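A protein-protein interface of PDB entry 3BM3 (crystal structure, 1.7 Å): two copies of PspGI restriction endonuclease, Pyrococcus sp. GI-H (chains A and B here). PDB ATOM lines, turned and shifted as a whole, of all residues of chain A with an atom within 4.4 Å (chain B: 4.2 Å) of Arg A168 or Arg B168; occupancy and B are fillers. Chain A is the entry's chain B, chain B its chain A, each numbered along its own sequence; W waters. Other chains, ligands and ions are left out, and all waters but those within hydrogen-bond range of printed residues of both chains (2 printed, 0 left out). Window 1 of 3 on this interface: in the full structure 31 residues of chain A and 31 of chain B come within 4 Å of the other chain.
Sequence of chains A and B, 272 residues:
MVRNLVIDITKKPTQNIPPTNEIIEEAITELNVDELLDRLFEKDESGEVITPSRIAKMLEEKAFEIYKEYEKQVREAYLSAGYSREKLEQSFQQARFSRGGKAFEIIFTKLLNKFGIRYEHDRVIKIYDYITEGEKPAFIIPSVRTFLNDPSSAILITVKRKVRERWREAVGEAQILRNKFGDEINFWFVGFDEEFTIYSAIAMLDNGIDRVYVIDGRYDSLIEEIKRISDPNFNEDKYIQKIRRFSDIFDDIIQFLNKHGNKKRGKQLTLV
Glu A165 touches Glu B169, and with the chains exchanged Glu A169 touches Glu B165. Arg A166 touches Glu B169, and with the chains exchanged Glu A169 touches Arg B166. Arg A168 touches its own counterpart, Arg B168. Val A171 touches Gly B172, and with the chains exchanged Gly A172 touches Val B171. Positions printed for both chains: 134, 135, 165, 166, 167, 168, 169, 170, 171, 172, 173 and 199. Of the 23 pairs that touch across the chains among the printed residues, 21 have their exchanged pair printed and touching as well.
Gly A134 touches Tyr B199 (C to OH, 3.5 Å). O of Gly B134 touches NH2 of Arg A168, at 3.7 Å. O of Arg A168 touches CA of Gly B172, at 3.6 Å. Glu A169 touches Arg B166. Arg B168 touches Glu A169. Gly B172 touches Val A171. Val B171 touches Gly A172 (CG1 to CA, 3.6 Å). Ile A176 touches Trp B167 (CD1 to CH2, 3.7 Å). Ile A176 touches Tyr B199. Gly B134 touches Tyr A199 (C to OH, 3.5 Å).
OE1 of Glu B135 is in salt-bridge range of NE of Arg A168 (2.7 Å). NE of Arg B168 lies within salt-bridge range of OE1 of Glu A135, 2.8 Å away. The side-chain carboxylate of Glu B135 is in hydrogen-bond range of the side-chain hydroxyl of Tyr A199 (2.5 Å). The backbone carbonyl oxygen of Arg A168 sits close to the backbone carbonyl oxygen of Arg B168 (3.3 Å). The side-chain hydroxyl (OH) of Tyr B199 is in hydrogen-bond range of the side-chain carboxylate (OE2) of Glu A135, at 2.5 Å. OE2 of Glu A169 sits close to OE2 of Glu B165. OE2 of Glu B169 lies close to OE2 of Glu A165 (2.6 Å).
Of the 12 printed residues of chain B, 10 touch a printed residue of chain A. Printed residues of chain B that touch a printed residue of chain A: Gly B134, Glu B135, Glu B165, Arg B166, Trp B167, Arg B168, Glu B169, Val B171, Gly B172 and Tyr B199. Of the 13 printed residues of chain A, 10 touch a printed residue of chain B. Hydrophobic or aromatic side chains of chain A within 4 Å of the printed part of chain B: Val A171, Ile A176 and Tyr A199.
Of the printed residues of chain B, Glu A165 touches Glu B169. Arg A168 touches just these residues of chain B: Gly B134 (3.7 Å), Glu B135 (2.7 Å), Arg B168 (3.3 Å), Glu B169 (3.8 Å) and Gly B172 (3.6 Å). Of the printed residues of chain A, Arg B168 touches Gly A134, Glu A135, Arg A168, Glu A169 and Gly A172. Printed residues of chain A within 4 Å of Val B171: Gly A172 (3.6 Å). The nearest printed residue of chain B that does not touch Arg A166 is Glu B165 (4.4 Å).
Water W2 bridges OE2 of Glu A165 (2.7 Å) and OE1 of Glu B169 (3.3 Å). Water W1 bridges the side-chain carboxylate of Glu B165 and the side-chain carboxylate of Glu A169.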
ATOM      1  N   GLY A 134      23.183  -7.228  19.297  1.00  0.00           N
ATOM      2  CA  GLY A 134      22.232  -6.697  20.258  1.00  0.00           C
ATOM      3  C   GLY A 134      22.425  -5.210  20.491  1.00  0.00           C
ATOM      4  O   GLY A 134      22.837  -4.447  19.607  1.00  0.00           O
ATOM      5  N   GLU A 135      22.121  -4.794  21.701  1.00  0.00           N
ATOM      6  CA  GLU A 135      22.256  -3.408  22.101  1.00  0.00           C
ATOM      7  C   GLU A 135      23.542  -3.277  22.905  1.00  0.00           C
ATOM      8  O   GLU A 135      23.878  -4.161  23.673  1.00  0.00           O
ATOM      9  CB  GLU A 135      21.046  -2.940  22.903  1.00  0.00           C
ATOM     10  CG  GLU A 135      19.782  -2.903  22.043  1.00  0.00           C
ATOM     11  CD  GLU A 135      19.967  -2.003  20.821  1.00  0.00           C
ATOM     12  OE1 GLU A 135      20.245  -0.799  21.023  1.00  0.00           O
ATOM     13  OE2 GLU A 135      19.897  -2.500  19.675  1.00  0.00           O
ATOM     14  N   GLU A 165      21.397  15.207  15.584  1.00  0.00           N
ATOM     15  CA  GLU A 165      20.102  14.519  15.702  1.00  0.00           C
ATOM     16  C   GLU A 165      20.253  13.122  16.296  1.00  0.00           C
ATOM     17  O   GLU A 165      19.277  12.378  16.481  1.00  0.00           O
ATOM     18  CB  GLU A 165      19.489  14.404  14.300  1.00  0.00           C
ATOM     19  CG  GLU A 165      19.940  13.232  13.426  1.00  0.00           C
ATOM     20  CD  GLU A 165      21.420  13.197  13.031  1.00  0.00           C
ATOM     21  OE1 GLU A 165      22.129  14.233  13.186  1.00  0.00           O
ATOM     22  OE2 GLU A 165      21.834  12.113  12.576  1.00  0.00           O
ATOM     23  N   ARG A 166      21.503  12.723  16.544  1.00  0.00           N
ATOM     24  CA  ARG A 166      21.802  11.378  16.958  1.00  0.00           C
ATOM     25  C   ARG A 166      21.315  10.959  18.332  1.00  0.00           C
ATOM     26  O   ARG A 166      21.326   9.782  18.690  1.00  0.00           O
ATOM     27  CB  ARG A 166      23.303  11.106  16.765  1.00  0.00           C
ATOM     28  CG  ARG A 166      23.673  11.020  15.310  1.00  0.00           C
ATOM     29  CD  ARG A 166      25.197  10.901  15.044  1.00  0.00           C
ATOM     30  NE  ARG A 166      25.814  12.219  15.172  1.00  0.00           N
ATOM     31  CZ  ARG A 166      26.381  12.712  16.270  1.00  0.00           C
ATOM     32  NH1 ARG A 166      26.525  11.981  17.372  1.00  0.00           N
ATOM     33  NH2 ARG A 166      26.820  13.949  16.240  1.00  0.00           N
ATOM     34  N   TRP A 167      20.834  11.934  19.109  1.00  0.00           N
ATOM     35  CA  TRP A 167      20.176  11.626  20.375  1.00  0.00           C
ATOM     36  C   TRP A 167      18.996  10.668  20.177  1.00  0.00           C
ATOM     37  O   TRP A 167      18.688   9.866  21.054  1.00  0.00           O
ATOM     38  CB  TRP A 167      19.668  12.906  21.039  1.00  0.00           C
ATOM     39  CG  TRP A 167      18.722  13.671  20.288  1.00  0.00           C
ATOM     40  CD1 TRP A 167      18.996  14.690  19.427  1.00  0.00           C
ATOM     41  CD2 TRP A 167      17.308  13.535  20.299  1.00  0.00           C
ATOM     42  NE1 TRP A 167      17.863  15.211  18.916  1.00  0.00           N
ATOM     43  CE2 TRP A 167      16.790  14.540  19.447  1.00  0.00           C
ATOM     44  CE3 TRP A 167      16.432  12.730  21.008  1.00  0.00           C
ATOM     45  CZ2 TRP A 167      15.426  14.709  19.237  1.00  0.00           C
ATOM     46  CZ3 TRP A 167      15.079  12.917  20.830  1.00  0.00           C
ATOM     47  CH2 TRP A 167      14.588  13.883  19.944  1.00  0.00           C
ATOM     48  N   ARG A 168      18.348  10.731  19.015  1.00  0.00           N
ATOM     49  CA  ARG A 168      17.266   9.767  18.770  1.00  0.00           C
ATOM     50  C   ARG A 168      17.745   8.323  18.787  1.00  0.00           C
ATOM     51  O   ARG A 168      16.971   7.417  19.070  1.00  0.00           O
ATOM     52  CB  ARG A 168      16.525  10.098  17.497  1.00  0.00           C
ATOM     53  CG  ARG A 168      15.639  11.327  17.595  1.00  0.00           C
ATOM     54  CD  ARG A 168      14.706  11.402  16.440  1.00  0.00           C
ATOM     55  NE  ARG A 168      13.951  12.651  16.440  1.00  0.00           N
ATOM     56  CZ  ARG A 168      14.446  13.840  16.136  1.00  0.00           C
ATOM     57  NH1 ARG A 168      15.714  13.976  15.739  1.00  0.00           N
ATOM     58  NH2 ARG A 168      13.675  14.918  16.182  1.00  0.00           N
ATOM     59  N   GLU A 169      19.038   8.095  18.532  1.00  0.00           N
ATOM     60  CA  GLU A 169      19.609   6.744  18.644  1.00  0.00           C
ATOM     61  C   GLU A 169      19.489   6.224  20.046  1.00  0.00           C
ATOM     62  O   GLU A 169      19.232   5.052  20.261  1.00  0.00           O
ATOM     63  CB  GLU A 169      21.055   6.702  18.227  1.00  0.00           C
ATOM     64  CG  GLU A 169      21.296   7.167  16.804  1.00  0.00           C
ATOM     65  CD  GLU A 169      22.741   7.146  16.420  1.00  0.00           C
ATOM     66  OE1 GLU A 169      23.593   7.047  17.314  1.00  0.00           O
ATOM     67  OE2 GLU A 169      22.984   7.159  15.195  1.00  0.00           O
ATOM     68  N   ALA A 170      19.635   7.118  21.016  1.00  0.00           N
ATOM     69  CA  ALA A 170      19.536   6.741  22.404  1.00  0.00           C
ATOM     70  C   ALA A 170      18.089   6.403  22.755  1.00  0.00           C
ATOM     71  O   ALA A 170      17.843   5.453  23.470  1.00  0.00           O
ATOM     72  CB  ALA A 170      20.034   7.847  23.275  1.00  0.00           C
ATOM     73  N   VAL A 171      17.143   7.188  22.241  1.00  0.00           N
ATOM     74  CA  VAL A 171      15.725   6.845  22.363  1.00  0.00           C
ATOM     75  C   VAL A 171      15.436   5.452  21.790  1.00  0.00           C
ATOM     76  O   VAL A 171      14.738   4.640  22.412  1.00  0.00           O
ATOM     77  CB  VAL A 171      14.835   7.933  21.763  1.00  0.00           C
ATOM     78  CG1 VAL A 171      13.362   7.544  21.898  1.00  0.00           C
ATOM     79  CG2 VAL A 171      15.066   9.277  22.443  1.00  0.00           C
ATOM     80  N   GLY A 172      15.984   5.173  20.607  1.00  0.00           N
ATOM     81  CA  GLY A 172      15.784   3.891  19.967  1.00  0.00           C
ATOM     82  C   GLY A 172      16.379   2.779  20.792  1.00  0.00           C
ATOM     83  O   GLY A 172      15.741   1.760  21.001  1.00  0.00           O
ATOM     84  N   GLU A 173      17.616   2.949  21.270  1.00  0.00           N
ATOM     85  CA  GLU A 173      18.247   1.927  22.092  1.00  0.00           C
ATOM     86  C   GLU A 173      17.432   1.689  23.351  1.00  0.00           C
ATOM     87  O   GLU A 173      17.132   0.573  23.727  1.00  0.00           O
ATOM     88  CB  GLU A 173      19.669   2.333  22.442  1.00  0.00           C
ATOM     89  CG  GLU A 173      20.365   1.368  23.316  1.00  0.00           C
ATOM     90  CD  GLU A 173      21.849   1.726  23.551  1.00  0.00           C
ATOM     91  OE1 GLU A 173      22.367   2.697  22.961  1.00  0.00           O
ATOM     92  OE2 GLU A 173      22.458   1.038  24.366  1.00  0.00           O
ATOM     93  N   ILE A 176      14.292  -0.318  22.518  1.00  0.00           N
ATOM     94  CA  ILE A 176      14.573  -1.732  22.308  1.00  0.00           C
ATOM     95  C   ILE A 176      14.799  -2.470  23.640  1.00  0.00           C
ATOM     96  O   ILE A 176      14.253  -3.572  23.894  1.00  0.00           O
ATOM     97  CB  ILE A 176      15.776  -1.925  21.403  1.00  0.00           C
ATOM     98  CG1 ILE A 176      15.462  -1.349  20.008  1.00  0.00           C
ATOM     99  CG2 ILE A 176      16.183  -3.404  21.384  1.00  0.00           C
ATOM    100  CD1 ILE A 176      16.666  -1.127  19.114  1.00  0.00           C
ATOM    101  N   TYR A 199      14.578  20.537  23.059  1.00  0.00           N
ATOM    102  CA  TYR A 199      13.649  19.529  22.576  1.00  0.00           C
ATOM    103  C   TYR A 199      14.222  18.141  22.754  1.00  0.00           C
ATOM    104  O   TYR A 199      13.523  17.226  23.165  1.00  0.00           O
ATOM    105  CB  TYR A 199      13.267  19.780  21.136  1.00  0.00           C
ATOM    106  CG  TYR A 199      12.400  18.702  20.549  1.00  0.00           C
ATOM    107  CD1 TYR A 199      11.035  18.637  20.845  1.00  0.00           C
ATOM    108  CD2 TYR A 199      12.940  17.733  19.723  1.00  0.00           C
ATOM    109  CE1 TYR A 199      10.239  17.635  20.339  1.00  0.00           C
ATOM    110  CE2 TYR A 199      12.156  16.725  19.175  1.00  0.00           C
ATOM    111  CZ  TYR A 199      10.786  16.684  19.501  1.00  0.00           C
ATOM    112  OH  TYR A 199       9.985  15.716  18.976  1.00  0.00           O
ATOM    113  N   GLY B 134       9.690  19.329  16.621  1.00  0.00           N
ATOM    114  CA  GLY B 134       8.964  18.080  16.631  1.00  0.00           C
ATOM    115  C   GLY B 134       9.652  17.043  15.793  1.00  0.00           C
ATOM    116  O   GLY B 134      10.848  17.135  15.511  1.00  0.00           O
ATOM    117  N   GLU B 135       8.890  16.035  15.415  1.00  0.00           N
ATOM    118  CA  GLU B 135       9.413  14.976  14.614  1.00  0.00           C
ATOM    119  C   GLU B 135       9.224  15.270  13.128  1.00  0.00           C
ATOM    120  O   GLU B 135       8.244  15.921  12.718  1.00  0.00           O
ATOM    121  CB  GLU B 135       8.823  13.654  15.027  1.00  0.00           C
ATOM    122  CG  GLU B 135       9.154  13.282  16.432  1.00  0.00           C
ATOM    123  CD  GLU B 135      10.657  13.241  16.662  1.00  0.00           C
ATOM    124  OE1 GLU B 135      11.312  12.404  16.047  1.00  0.00           O
ATOM    125  OE2 GLU B 135      11.155  14.101  17.417  1.00  0.00           O
ATOM    126  N   GLU B 165      24.503   2.849  12.183  1.00  0.00           N
ATOM    127  CA  GLU B 165      23.741   2.674  13.395  1.00  0.00           C
ATOM    128  C   GLU B 165      22.514   3.593  13.441  1.00  0.00           C
ATOM    129  O   GLU B 165      21.755   3.565  14.403  1.00  0.00           O
ATOM    130  CB  GLU B 165      24.636   2.957  14.618  1.00  0.00           C
ATOM    131  CG  GLU B 165      24.739   4.358  15.080  1.00  0.00           C
ATOM    132  CD  GLU B 165      25.425   5.345  14.115  1.00  0.00           C
ATOM    133  OE1 GLU B 165      26.038   4.917  13.124  1.00  0.00           O
ATOM    134  OE2 GLU B 165      25.317   6.555  14.366  1.00  0.00           O
ATOM    135  N   ARG B 166      22.375   4.484  12.457  1.00  0.00           N
ATOM    136  CA  ARG B 166      21.414   5.567  12.488  1.00  0.00           C
ATOM    137  C   ARG B 166      19.965   5.118  12.358  1.00  0.00           C
ATOM    138  O   ARG B 166      19.028   5.888  12.549  1.00  0.00           O
ATOM    139  CB  ARG B 166      21.808   6.626  11.439  1.00  0.00           C
ATOM    140  CG  ARG B 166      23.056   7.397  11.850  1.00  0.00           C
ATOM    141  CD  ARG B 166      23.505   8.377  10.808  1.00  0.00           C
ATOM    142  NE  ARG B 166      24.320   7.696   9.834  1.00  0.00           N
ATOM    143  CZ  ARG B 166      23.903   7.219   8.671  1.00  0.00           C
ATOM    144  NH1 ARG B 166      22.663   7.402   8.227  1.00  0.00           N
ATOM    145  NH2 ARG B 166      24.765   6.553   7.939  1.00  0.00           N
ATOM    146  N   TRP B 167      19.766   3.855  12.014  1.00  0.00           N
ATOM    147  CA  TRP B 167      18.436   3.270  12.062  1.00  0.00           C
ATOM    148  C   TRP B 167      17.792   3.427  13.422  1.00  0.00           C
ATOM    149  O   TRP B 167      16.588   3.509  13.504  1.00  0.00           O
ATOM    150  CB  TRP B 167      18.463   1.800  11.689  1.00  0.00           C
ATOM    151  CG  TRP B 167      19.233   0.938  12.529  1.00  0.00           C
ATOM    152  CD1 TRP B 167      20.556   0.603  12.367  1.00  0.00           C
ATOM    153  CD2 TRP B 167      18.773   0.223  13.650  1.00  0.00           C
ATOM    154  NE1 TRP B 167      20.936  -0.278  13.335  1.00  0.00           N
ATOM    155  CE2 TRP B 167      19.856  -0.530  14.140  1.00  0.00           C
ATOM    156  CE3 TRP B 167      17.538   0.141  14.304  1.00  0.00           C
ATOM    157  CZ2 TRP B 167      19.735  -1.353  15.257  1.00  0.00           C
ATOM    158  CZ3 TRP B 167      17.419  -0.697  15.375  1.00  0.00           C
ATOM    159  CH2 TRP B 167      18.511  -1.406  15.872  1.00  0.00           C
ATOM    160  N   ARG B 168      18.583   3.458  14.497  1.00  0.00           N
ATOM    161  CA  ARG B 168      17.974   3.653  15.813  1.00  0.00           C
ATOM    162  C   ARG B 168      17.285   5.019  15.926  1.00  0.00           C
ATOM    163  O   ARG B 168      16.412   5.180  16.748  1.00  0.00           O
ATOM    164  CB  ARG B 168      18.965   3.446  16.940  1.00  0.00           C
ATOM    165  CG  ARG B 168      19.396   1.999  17.068  1.00  0.00           C
ATOM    166  CD  ARG B 168      20.114   1.765  18.372  1.00  0.00           C
ATOM    167  NE  ARG B 168      20.553   0.379  18.497  1.00  0.00           N
ATOM    168  CZ  ARG B 168      21.598  -0.132  17.869  1.00  0.00           C
ATOM    169  NH1 ARG B 168      22.391   0.647  17.124  1.00  0.00           N
ATOM    170  NH2 ARG B 168      21.911  -1.410  18.027  1.00  0.00           N
ATOM    171  N   GLU B 169      17.695   6.000  15.104  1.00  0.00           N
ATOM    172  CA  GLU B 169      17.026   7.279  15.039  1.00  0.00           C
ATOM    173  C   GLU B 169      15.577   7.085  14.649  1.00  0.00           C
ATOM    174  O   GLU B 169      14.709   7.755  15.157  1.00  0.00           O
ATOM    175  CB  GLU B 169      17.665   8.214  14.055  1.00  0.00           C
ATOM    176  CG  GLU B 169      19.064   8.635  14.474  1.00  0.00           C
ATOM    177  CD  GLU B 169      19.746   9.532  13.480  1.00  0.00           C
ATOM    178  OE1 GLU B 169      19.221   9.704  12.360  1.00  0.00           O
ATOM    179  OE2 GLU B 169      20.802  10.057  13.875  1.00  0.00           O
ATOM    180  N   ALA B 170      15.349   6.147  13.730  1.00  0.00           N
ATOM    181  CA  ALA B 170      13.992   5.889  13.246  1.00  0.00           C
ATOM    182  C   ALA B 170      13.166   5.249  14.346  1.00  0.00           C
ATOM    183  O   ALA B 170      11.989   5.600  14.514  1.00  0.00           O
ATOM    184  CB  ALA B 170      14.041   5.009  12.032  1.00  0.00           C
ATOM    185  N   VAL B 171      13.774   4.347  15.116  1.00  0.00           N
ATOM    186  CA  VAL B 171      13.116   3.693  16.242  1.00  0.00           C
ATOM    187  C   VAL B 171      12.771   4.786  17.249  1.00  0.00           C
ATOM    188  O   VAL B 171      11.677   4.846  17.746  1.00  0.00           O
ATOM    189  CB  VAL B 171      13.969   2.613  16.884  1.00  0.00           C
ATOM    190  CG1 VAL B 171      13.280   2.020  18.133  1.00  0.00           C
ATOM    191  CG2 VAL B 171      14.327   1.481  15.887  1.00  0.00           C
ATOM    192  N   GLY B 172      13.696   5.712  17.451  1.00  0.00           N
ATOM    193  CA  GLY B 172      13.493   6.844  18.359  1.00  0.00           C
ATOM    194  C   GLY B 172      12.351   7.711  17.908  1.00  0.00           C
ATOM    195  O   GLY B 172      11.450   8.045  18.684  1.00  0.00           O
ATOM    196  N   GLU B 173      12.369   8.093  16.633  1.00  0.00           N
ATOM    197  CA  GLU B 173      11.323   8.905  16.066  1.00  0.00           C
ATOM    198  C   GLU B 173       9.948   8.219  16.215  1.00  0.00           C
ATOM    199  O   GLU B 173       8.950   8.813  16.636  1.00  0.00           O
ATOM    200  CB  GLU B 173      11.623   9.204  14.603  1.00  0.00           C
ATOM    201  CG  GLU B 173      10.590  10.057  13.983  1.00  0.00           C
ATOM    202  CD  GLU B 173      10.864  10.391  12.549  1.00  0.00           C
ATOM    203  OE1 GLU B 173      11.939  10.031  12.036  1.00  0.00           O
ATOM    204  OE2 GLU B 173       9.964  10.974  11.927  1.00  0.00           O
ATOM    205  N   TYR B 199      19.795  -7.510  12.028  1.00  0.00           N
ATOM    206  CA  TYR B 199      19.413  -7.073  13.369  1.00  0.00           C
ATOM    207  C   TYR B 199      18.593  -5.804  13.260  1.00  0.00           C
ATOM    208  O   TYR B 199      17.563  -5.678  13.914  1.00  0.00           O
ATOM    209  CB  TYR B 199      20.598  -6.853  14.285  1.00  0.00           C
ATOM    210  CG  TYR B 199      20.203  -6.341  15.629  1.00  0.00           C
ATOM    211  CD1 TYR B 199      19.591  -7.165  16.545  1.00  0.00           C
ATOM    212  CD2 TYR B 199      20.469  -5.020  16.005  1.00  0.00           C
ATOM    213  CE1 TYR B 199      19.203  -6.683  17.789  1.00  0.00           C
ATOM    214  CE2 TYR B 199      20.124  -4.552  17.235  1.00  0.00           C
ATOM    215  CZ  TYR B 199      19.475  -5.374  18.131  1.00  0.00           C
ATOM    216  OH  TYR B 199      19.146  -4.871  19.364  1.00  0.00           O
HETATM  217  O   HOH W   1      26.813   6.871  16.634  1.00  0.00           O
HETATM  218  O   HOH W   2      20.502  11.896  10.209  1.00  0.00           O
